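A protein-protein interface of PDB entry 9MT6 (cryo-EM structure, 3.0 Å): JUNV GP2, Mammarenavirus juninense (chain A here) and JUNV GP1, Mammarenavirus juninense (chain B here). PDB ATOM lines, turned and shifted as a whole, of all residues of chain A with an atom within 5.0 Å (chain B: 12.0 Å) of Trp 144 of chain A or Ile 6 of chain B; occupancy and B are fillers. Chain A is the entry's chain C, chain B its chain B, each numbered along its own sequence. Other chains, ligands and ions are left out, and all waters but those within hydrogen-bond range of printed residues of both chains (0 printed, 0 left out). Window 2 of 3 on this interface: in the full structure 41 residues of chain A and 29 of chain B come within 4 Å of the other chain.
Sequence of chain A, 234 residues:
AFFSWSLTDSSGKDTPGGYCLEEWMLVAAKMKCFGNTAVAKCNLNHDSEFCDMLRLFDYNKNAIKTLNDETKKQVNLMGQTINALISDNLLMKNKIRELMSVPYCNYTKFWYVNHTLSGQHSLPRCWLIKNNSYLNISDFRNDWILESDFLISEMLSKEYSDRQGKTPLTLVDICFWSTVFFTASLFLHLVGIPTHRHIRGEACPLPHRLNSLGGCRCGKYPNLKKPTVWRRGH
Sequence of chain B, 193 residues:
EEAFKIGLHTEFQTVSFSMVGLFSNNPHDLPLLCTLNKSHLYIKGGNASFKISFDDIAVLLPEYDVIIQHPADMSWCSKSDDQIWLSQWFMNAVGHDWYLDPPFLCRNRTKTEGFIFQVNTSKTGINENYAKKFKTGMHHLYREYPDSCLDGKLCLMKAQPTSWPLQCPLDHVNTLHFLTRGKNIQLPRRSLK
The side-chain hydroxyl (OG) of Ser 148 of chain A is in hydrogen-bond range of the side-chain hydroxyl (OG1) of Thr 10 of chain B.
N of Gly 7 of chain B is in hydrogen-bond range of OG1 of Thr 10 of chain B. The indole nitrogen of Trp 144 of chain A lies close to the backbone carbonyl oxygen of Ile 137 of chain A (3.3 Å). O of Phe 140 of chain A lies close to NE1 of Trp 144 of chain A, 3.4 Å away. The backbone carbonyl oxygen (O) of Phe 4 of chain B lies within hydrogen-bond range of the backbone NH (N) of Phe 12 of chain B (2.8 Å).
Among the printed residues, merely in contact across the chains: Trp 111 of chain A with Gln 13 of chain B, Trp 144 of chain A with Ile 6 of chain B, Trp 111 of chain A with Phe 12 of chain B, Ser 148 of chain A with Ile 6 of chain B, Val 113 of chain A with Glu 11 of chain B, Trp 144 of chain A with Phe 4 of chain B, Val 113 of chain A with Ile 6 of chain B, Val 113 of chain A with Thr 10 of chain B, Ile 137 of chain A with Phe 4 of chain B, Phe 140 of chain A with Phe 12 of chain B, Trp 144 of chain A with Phe 12 of chain B and Trp 111 of chain A with Thr 14 of chain B.
Of the printed residues of chain B, Trp 111 of chain A touches Phe 12, Gln 13 and Thr 14. Of the printed residues of chain B, Val 113 of chain A touches Ile 6 (3.7 Å), Thr 10 (3.8 Å) and Glu 11 (3.6 Å). Ile 137 of chain A touches one residue of chain B. Phe 140 of chain A touches one residue of chain B. No residue of chain B comes within 4 Å of Arg 141 of chain A. No residue of chain B comes within 4 Å of Asn 142 of chain A. Asp 143 of chain A touches none of the printed residues of chain B. Of chain B, only Phe 4 (3.6 Å), Ile 6 (3.4 Å) and Phe 12 (3.9 Å) come within 4 Å of Trp 144 of chain A. No residue of chain B comes within 4 Å of Ile 145 of chain A. No residue of chain B comes within 4 Å of Glu 147 of chain A. Of the printed residues of chain B, Ser 148 of chain A touches Ile 6 and Thr 10. Printed residues of chain A within 4 Å of Glu 11 of chain B: Val 113 (3.6 Å). Of the printed residues of chain A, Phe 12 of chain B touches Trp 111, Phe 140 and Trp 144. Of the printed residues of chain A, Gln 13 of chain B touches Trp 111 (3.3 Å). Printed residues of chain A within 4 Å of Thr 14 of chain B: Trp 111. The nearest printed residue of chain A that does not touch Thr 14 of chain B is Val 113 of chain A (7.1 Å).
Hydrophobic or aromatic side chains of chain B that line the printed part of chain A: Phe 4, Ile 6 and Phe 12. Along chain B the printed residues that touch a printed residue of chain A span positions 4 to 14. Hydrophobic or aromatic side chains of chain A that line the printed part of chain B: Trp 111, Val 113, Ile 137, Phe 140 and Trp 144. Along chain A the printed residues that touch a printed residue of chain B span positions 111 to 148.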
ATOM      1  N   TRP A 111      13.220  27.073 -11.494  1.00  0.00           N
ATOM      2  CA  TRP A 111      11.873  26.702 -11.094  1.00  0.00           C
ATOM      3  C   TRP A 111      11.773  25.193 -10.935  1.00  0.00           C
ATOM      4  O   TRP A 111      12.494  24.432 -11.583  1.00  0.00           O
ATOM      5  CB  TRP A 111      10.827  27.187 -12.101  1.00  0.00           C
ATOM      6  CG  TRP A 111      10.943  26.575 -13.456  1.00  0.00           C
ATOM      7  CD1 TRP A 111      11.573  27.103 -14.538  1.00  0.00           C
ATOM      8  CD2 TRP A 111      10.406  25.316 -13.878  1.00  0.00           C
ATOM      9  NE1 TRP A 111      11.466  26.253 -15.610  1.00  0.00           N
ATOM     10  CE2 TRP A 111      10.753  25.148 -15.229  1.00  0.00           C
ATOM     11  CE3 TRP A 111       9.667  24.316 -13.243  1.00  0.00           C
ATOM     12  CZ2 TRP A 111      10.390  24.022 -15.953  1.00  0.00           C
ATOM     13  CZ3 TRP A 111       9.309  23.201 -13.964  1.00  0.00           C
ATOM     14  CH2 TRP A 111       9.669  23.063 -15.304  1.00  0.00           C
ATOM     15  N   VAL A 113       8.813  21.875  -9.383  1.00  0.00           N
ATOM     16  CA  VAL A 113       7.479  21.457  -8.968  1.00  0.00           C
ATOM     17  C   VAL A 113       7.615  20.691  -7.663  1.00  0.00           C
ATOM     18  O   VAL A 113       8.404  19.742  -7.572  1.00  0.00           O
ATOM     19  CB  VAL A 113       6.795  20.602 -10.045  1.00  0.00           C
ATOM     20  CG1 VAL A 113       5.530  19.973  -9.496  1.00  0.00           C
ATOM     21  CG2 VAL A 113       6.493  21.444 -11.267  1.00  0.00           C
ATOM     22  N   ILE A 137       5.300  32.203 -18.000  1.00  0.00           N
ATOM     23  CA  ILE A 137       4.962  30.853 -17.561  1.00  0.00           C
ATOM     24  C   ILE A 137       4.258  30.085 -18.674  1.00  0.00           C
ATOM     25  O   ILE A 137       4.400  28.861 -18.795  1.00  0.00           O
ATOM     26  CB  ILE A 137       4.108  30.916 -16.282  1.00  0.00           C
ATOM     27  CG1 ILE A 137       4.734  31.876 -15.275  1.00  0.00           C
ATOM     28  CG2 ILE A 137       3.977  29.549 -15.654  1.00  0.00           C
ATOM     29  CD1 ILE A 137       3.847  32.172 -14.094  1.00  0.00           C
ATOM     30  N   PHE A 140       6.581  27.774 -21.155  1.00  0.00           N
ATOM     31  CA  PHE A 140       6.969  26.448 -20.688  1.00  0.00           C
ATOM     32  C   PHE A 140       5.898  25.829 -19.791  1.00  0.00           C
ATOM     33  O   PHE A 140       6.207  25.049 -18.882  1.00  0.00           O
ATOM     34  CB  PHE A 140       8.323  26.495 -19.978  1.00  0.00           C
ATOM     35  CG  PHE A 140       8.387  27.459 -18.826  1.00  0.00           C
ATOM     36  CD1 PHE A 140       8.543  28.813 -19.044  1.00  0.00           C
ATOM     37  CD2 PHE A 140       8.311  27.004 -17.524  1.00  0.00           C
ATOM     38  CE1 PHE A 140       8.609  29.693 -17.991  1.00  0.00           C
ATOM     39  CE2 PHE A 140       8.376  27.884 -16.467  1.00  0.00           C
ATOM     40  CZ  PHE A 140       8.526  29.230 -16.704  1.00  0.00           C
ATOM     41  N   ARG A 141       4.636  26.196 -20.030  1.00  0.00           N
ATOM     42  CA  ARG A 141       3.518  25.508 -19.392  1.00  0.00           C
ATOM     43  C   ARG A 141       3.581  24.007 -19.638  1.00  0.00           C
ATOM     44  O   ARG A 141       3.374  23.205 -18.718  1.00  0.00           O
ATOM     45  CB  ARG A 141       2.195  26.075 -19.901  1.00  0.00           C
ATOM     46  CG  ARG A 141       0.977  25.357 -19.365  1.00  0.00           C
ATOM     47  CD  ARG A 141      -0.303  25.962 -19.907  1.00  0.00           C
ATOM     48  NE  ARG A 141      -1.482  25.394 -19.268  1.00  0.00           N
ATOM     49  CZ  ARG A 141      -1.996  24.207 -19.564  1.00  0.00           C
ATOM     50  NH1 ARG A 141      -1.456  23.434 -20.492  1.00  0.00           N
ATOM     51  NH2 ARG A 141      -3.077  23.787 -18.915  1.00  0.00           N
ATOM     52  N   ASN A 142       3.862  23.608 -20.879  1.00  0.00           N
ATOM     53  CA  ASN A 142       4.015  22.188 -21.175  1.00  0.00           C
ATOM     54  C   ASN A 142       5.161  21.589 -20.377  1.00  0.00           C
ATOM     55  O   ASN A 142       5.052  20.472 -19.855  1.00  0.00           O
ATOM     56  CB  ASN A 142       4.242  21.983 -22.672  1.00  0.00           C
ATOM     57  CG  ASN A 142       4.326  20.519 -23.051  1.00  0.00           C
ATOM     58  OD1 ASN A 142       3.672  19.671 -22.444  1.00  0.00           O
ATOM     59  ND2 ASN A 142       5.138  20.213 -24.055  1.00  0.00           N
ATOM     60  N   ASP A 143       6.265  22.331 -20.259  1.00  0.00           N
ATOM     61  CA  ASP A 143       7.423  21.838 -19.525  1.00  0.00           C
ATOM     62  C   ASP A 143       7.071  21.551 -18.073  1.00  0.00           C
ATOM     63  O   ASP A 143       7.371  20.469 -17.555  1.00  0.00           O
ATOM     64  CB  ASP A 143       8.566  22.847 -19.616  1.00  0.00           C
ATOM     65  CG  ASP A 143       9.462  22.605 -20.811  1.00  0.00           C
ATOM     66  OD1 ASP A 143       9.569  21.440 -21.248  1.00  0.00           O
ATOM     67  OD2 ASP A 143      10.054  23.579 -21.318  1.00  0.00           O
ATOM     68  N   TRP A 144       6.407  22.491 -17.397  1.00  0.00           N
ATOM     69  CA  TRP A 144       6.138  22.223 -15.987  1.00  0.00           C
ATOM     70  C   TRP A 144       4.958  21.282 -15.767  1.00  0.00           C
ATOM     71  O   TRP A 144       4.928  20.591 -14.743  1.00  0.00           O
ATOM     72  CB  TRP A 144       5.952  23.504 -15.162  1.00  0.00           C
ATOM     73  CG  TRP A 144       5.026  24.568 -15.638  1.00  0.00           C
ATOM     74  CD1 TRP A 144       5.378  25.736 -16.235  1.00  0.00           C
ATOM     75  CD2 TRP A 144       3.608  24.628 -15.448  1.00  0.00           C
ATOM     76  NE1 TRP A 144       4.269  26.498 -16.479  1.00  0.00           N
ATOM     77  CE2 TRP A 144       3.166  25.843 -16.002  1.00  0.00           C
ATOM     78  CE3 TRP A 144       2.666  23.761 -14.889  1.00  0.00           C
ATOM     79  CZ2 TRP A 144       1.827  26.215 -16.018  1.00  0.00           C
ATOM     80  CZ3 TRP A 144       1.334  24.132 -14.908  1.00  0.00           C
ATOM     81  CH2 TRP A 144       0.928  25.349 -15.465  1.00  0.00           C
ATOM     82  N   ILE A 145       4.014  21.191 -16.708  1.00  0.00           N
ATOM     83  CA  ILE A 145       2.985  20.159 -16.606  1.00  0.00           C
ATOM     84  C   ILE A 145       3.619  18.775 -16.698  1.00  0.00           C
ATOM     85  O   ILE A 145       3.327  17.877 -15.893  1.00  0.00           O
ATOM     86  CB  ILE A 145       1.909  20.363 -17.687  1.00  0.00           C
ATOM     87  CG1 ILE A 145       0.922  21.445 -17.252  1.00  0.00           C
ATOM     88  CG2 ILE A 145       1.182  19.061 -17.976  1.00  0.00           C
ATOM     89  CD1 ILE A 145       0.038  21.031 -16.101  1.00  0.00           C
ATOM     90  N   LEU A 146       4.509  18.588 -17.675  1.00  0.00           N
ATOM     91  CA  LEU A 146       5.214  17.318 -17.795  1.00  0.00           C
ATOM     92  C   LEU A 146       6.090  17.065 -16.575  1.00  0.00           C
ATOM     93  O   LEU A 146       6.239  15.920 -16.142  1.00  0.00           O
ATOM     94  CB  LEU A 146       6.042  17.302 -19.080  1.00  0.00           C
ATOM     95  CG  LEU A 146       6.701  15.996 -19.531  1.00  0.00           C
ATOM     96  CD1 LEU A 146       6.809  15.975 -21.045  1.00  0.00           C
ATOM     97  CD2 LEU A 146       8.079  15.812 -18.911  1.00  0.00           C
ATOM     98  N   GLU A 147       6.676  18.122 -16.006  1.00  0.00           N
ATOM     99  CA  GLU A 147       7.488  17.958 -14.805  1.00  0.00           C
ATOM    100  C   GLU A 147       6.649  17.472 -13.628  1.00  0.00           C
ATOM    101  O   GLU A 147       7.078  16.590 -12.876  1.00  0.00           O
ATOM    102  CB  GLU A 147       8.185  19.275 -14.460  1.00  0.00           C
ATOM    103  CG  GLU A 147       9.543  19.124 -13.789  1.00  0.00           C
ATOM    104  CD  GLU A 147      10.567  18.395 -14.642  1.00  0.00           C
ATOM    105  OE1 GLU A 147      10.357  18.256 -15.865  1.00  0.00           O
ATOM    106  OE2 GLU A 147      11.591  17.955 -14.079  1.00  0.00           O
ATOM    107  N   SER A 148       5.452  18.034 -13.449  1.00  0.00           N
ATOM    108  CA  SER A 148       4.572  17.580 -12.375  1.00  0.00           C
ATOM    109  C   SER A 148       4.151  16.128 -12.581  1.00  0.00           C
ATOM    110  O   SER A 148       4.153  15.323 -11.637  1.00  0.00           O
ATOM    111  CB  SER A 148       3.345  18.482 -12.287  1.00  0.00           C
ATOM    112  OG  SER A 148       2.457  18.037 -11.278  1.00  0.00           O
ATOM    113  N   GLU B   2       6.354  33.459  -9.746  1.00  0.00           N
ATOM    114  CA  GLU B   2       5.547  33.404  -8.534  1.00  0.00           C
ATOM    115  C   GLU B   2       5.023  31.992  -8.309  1.00  0.00           C
ATOM    116  O   GLU B   2       4.801  31.245  -9.261  1.00  0.00           O
ATOM    117  CB  GLU B   2       4.387  34.400  -8.614  1.00  0.00           C
ATOM    118  CG  GLU B   2       3.711  34.703  -7.282  1.00  0.00           C
ATOM    119  CD  GLU B   2       4.691  35.146  -6.209  1.00  0.00           C
ATOM    120  OE1 GLU B   2       5.223  34.278  -5.486  1.00  0.00           O
ATOM    121  OE2 GLU B   2       4.933  36.365  -6.095  1.00  0.00           O
ATOM    122  N   ALA B   3       4.826  31.629  -7.044  1.00  0.00           N
ATOM    123  CA  ALA B   3       4.364  30.293  -6.702  1.00  0.00           C
ATOM    124  C   ALA B   3       2.870  30.157  -6.957  1.00  0.00           C
ATOM    125  O   ALA B   3       2.075  31.005  -6.544  1.00  0.00           O
ATOM    126  CB  ALA B   3       4.676  29.978  -5.240  1.00  0.00           C
ATOM    127  N   PHE B   4       2.490  29.081  -7.640  1.00  0.00           N
ATOM    128  CA  PHE B   4       1.083  28.813  -7.894  1.00  0.00           C
ATOM    129  C   PHE B   4       0.877  27.312  -8.013  1.00  0.00           C
ATOM    130  O   PHE B   4       1.767  26.576  -8.446  1.00  0.00           O
ATOM    131  CB  PHE B   4       0.590  29.541  -9.150  1.00  0.00           C
ATOM    132  CG  PHE B   4       1.102  28.961 -10.436  1.00  0.00           C
ATOM    133  CD1 PHE B   4       2.394  29.202 -10.855  1.00  0.00           C
ATOM    134  CD2 PHE B   4       0.274  28.203 -11.244  1.00  0.00           C
ATOM    135  CE1 PHE B   4       2.860  28.679 -12.040  1.00  0.00           C
ATOM    136  CE2 PHE B   4       0.735  27.683 -12.433  1.00  0.00           C
ATOM    137  CZ  PHE B   4       2.030  27.917 -12.830  1.00  0.00           C
ATOM    138  N   LYS B   5      -0.316  26.869  -7.626  1.00  0.00           N
ATOM    139  CA  LYS B   5      -0.643  25.451  -7.648  1.00  0.00           C
ATOM    140  C   LYS B   5      -0.940  24.991  -9.065  1.00  0.00           C
ATOM    141  O   LYS B   5      -1.586  25.699  -9.842  1.00  0.00           O
ATOM    142  CB  LYS B   5      -1.841  25.159  -6.745  1.00  0.00           C
ATOM    143  CG  LYS B   5      -1.585  25.423  -5.274  1.00  0.00           C
ATOM    144  CD  LYS B   5      -2.849  25.257  -4.455  1.00  0.00           C
ATOM    145  CE  LYS B   5      -2.628  25.684  -3.014  1.00  0.00           C
ATOM    146  NZ  LYS B   5      -3.896  25.680  -2.234  1.00  0.00           N
ATOM    147  N   ILE B   6      -0.459  23.797  -9.398  1.00  0.00           N
ATOM    148  CA  ILE B   6      -0.673  23.228 -10.720  1.00  0.00           C
ATOM    149  C   ILE B   6      -1.368  21.877 -10.678  1.00  0.00           C
ATOM    150  O   ILE B   6      -1.804  21.389 -11.733  1.00  0.00           O
ATOM    151  CB  ILE B   6       0.655  23.122 -11.496  1.00  0.00           C
ATOM    152  CG1 ILE B   6       1.602  22.143 -10.823  1.00  0.00           C
ATOM    153  CG2 ILE B   6       1.343  24.466 -11.540  1.00  0.00           C
ATOM    154  CD1 ILE B   6       2.843  21.897 -11.633  1.00  0.00           C
ATOM    155  N   GLY B   7      -1.486  21.250  -9.511  1.00  0.00           N
ATOM    156  CA  GLY B   7      -2.257  20.035  -9.354  1.00  0.00           C
ATOM    157  C   GLY B   7      -3.024  20.053  -8.049  1.00  0.00           C
ATOM    158  O   GLY B   7      -3.382  21.126  -7.557  1.00  0.00           O
ATOM    159  N   LEU B   8      -3.289  18.879  -7.477  1.00  0.00           N
ATOM    160  CA  LEU B   8      -3.954  18.836  -6.179  1.00  0.00           C
ATOM    161  C   LEU B   8      -3.024  19.312  -5.071  1.00  0.00           C
ATOM    162  O   LEU B   8      -3.408  20.141  -4.239  1.00  0.00           O
ATOM    163  CB  LEU B   8      -4.458  17.424  -5.888  1.00  0.00           C
ATOM    164  CG  LEU B   8      -5.311  17.324  -4.621  1.00  0.00           C
ATOM    165  CD1 LEU B   8      -6.523  18.237  -4.718  1.00  0.00           C
ATOM    166  CD2 LEU B   8      -5.735  15.894  -4.360  1.00  0.00           C
ATOM    167  N   HIS B   9      -1.796  18.797  -5.043  1.00  0.00           N
ATOM    168  CA  HIS B   9      -0.791  19.233  -4.085  1.00  0.00           C
ATOM    169  C   HIS B   9       0.472  19.777  -4.728  1.00  0.00           C
ATOM    170  O   HIS B   9       1.230  20.479  -4.049  1.00  0.00           O
ATOM    171  CB  HIS B   9      -0.396  18.081  -3.146  1.00  0.00           C
ATOM    172  CG  HIS B   9      -1.529  17.175  -2.785  1.00  0.00           C
ATOM    173  ND1 HIS B   9      -2.558  17.564  -1.955  1.00  0.00           N
ATOM    174  CD2 HIS B   9      -1.792  15.893  -3.133  1.00  0.00           C
ATOM    175  CE1 HIS B   9      -3.408  16.563  -1.811  1.00  0.00           C
ATOM    176  NE2 HIS B   9      -2.966  15.537  -2.516  1.00  0.00           N
ATOM    177  N   THR B  10       0.726  19.478  -5.999  1.00  0.00           N
ATOM    178  CA  THR B  10       1.923  19.962  -6.668  1.00  0.00           C
ATOM    179  C   THR B  10       1.828  21.467  -6.867  1.00  0.00           C
ATOM    180  O   THR B  10       0.807  21.976  -7.339  1.00  0.00           O
ATOM    181  CB  THR B  10       2.110  19.260  -8.010  1.00  0.00           C
ATOM    182  OG1 THR B  10       0.923  19.408  -8.798  1.00  0.00           O
ATOM    183  CG2 THR B  10       2.387  17.785  -7.800  1.00  0.00           C
ATOM    184  N   GLU B  11       2.892  22.176  -6.506  1.00  0.00           N
ATOM    185  CA  GLU B  11       2.935  23.628  -6.593  1.00  0.00           C
ATOM    186  C   GLU B  11       4.186  24.057  -7.344  1.00  0.00           C
ATOM    187  O   GLU B  11       5.288  23.582  -7.048  1.00  0.00           O
ATOM    188  CB  GLU B  11       2.907  24.260  -5.201  1.00  0.00           C
ATOM    189  CG  GLU B  11       2.213  25.608  -5.153  1.00  0.00           C
ATOM    190  CD  GLU B  11       2.096  26.154  -3.744  1.00  0.00           C
ATOM    191  OE1 GLU B  11       2.193  25.357  -2.789  1.00  0.00           O
ATOM    192  OE2 GLU B  11       1.909  27.379  -3.594  1.00  0.00           O
ATOM    193  N   PHE B  12       4.010  24.952  -8.309  1.00  0.00           N
ATOM    194  CA  PHE B  12       5.130  25.517  -9.048  1.00  0.00           C
ATOM    195  C   PHE B  12       5.867  26.510  -8.158  1.00  0.00           C
ATOM    196  O   PHE B  12       5.285  27.503  -7.714  1.00  0.00           O
ATOM    197  CB  PHE B  12       4.611  26.188 -10.316  1.00  0.00           C
ATOM    198  CG  PHE B  12       5.670  26.843 -11.153  1.00  0.00           C
ATOM    199  CD1 PHE B  12       6.024  28.162 -10.940  1.00  0.00           C
ATOM    200  CD2 PHE B  12       6.281  26.154 -12.180  1.00  0.00           C
ATOM    201  CE1 PHE B  12       6.982  28.766 -11.716  1.00  0.00           C
ATOM    202  CE2 PHE B  12       7.240  26.759 -12.960  1.00  0.00           C
ATOM    203  CZ  PHE B  12       7.588  28.066 -12.728  1.00  0.00           C
ATOM    204  N   GLN B  13       7.143  26.244  -7.893  1.00  0.00           N
ATOM    205  CA  GLN B  13       7.939  27.053  -6.984  1.00  0.00           C
ATOM    206  C   GLN B  13       9.260  27.416  -7.647  1.00  0.00           C
ATOM    207  O   GLN B  13       9.734  26.714  -8.543  1.00  0.00           O
ATOM    208  CB  GLN B  13       8.200  26.318  -5.665  1.00  0.00           C
ATOM    209  CG  GLN B  13       6.962  25.694  -5.053  1.00  0.00           C
ATOM    210  CD  GLN B  13       7.080  25.506  -3.560  1.00  0.00           C
ATOM    211  OE1 GLN B  13       8.063  24.954  -3.069  1.00  0.00           O
ATOM    212  NE2 GLN B  13       6.075  25.966  -2.826  1.00  0.00           N
ATOM    213  N   THR B  14       9.852  28.523  -7.200  1.00  0.00           N
ATOM    214  CA  THR B  14      11.053  29.065  -7.818  1.00  0.00           C
ATOM    215  C   THR B  14      12.110  29.377  -6.770  1.00  0.00           C
ATOM    216  O   THR B  14      11.799  29.753  -5.638  1.00  0.00           O
ATOM    217  CB  THR B  14      10.753  30.339  -8.616  1.00  0.00           C
ATOM    218  OG1 THR B  14      10.263  31.353  -7.732  1.00  0.00           O
ATOM    219  CG2 THR B  14       9.715  30.067  -9.688  1.00  0.00           C
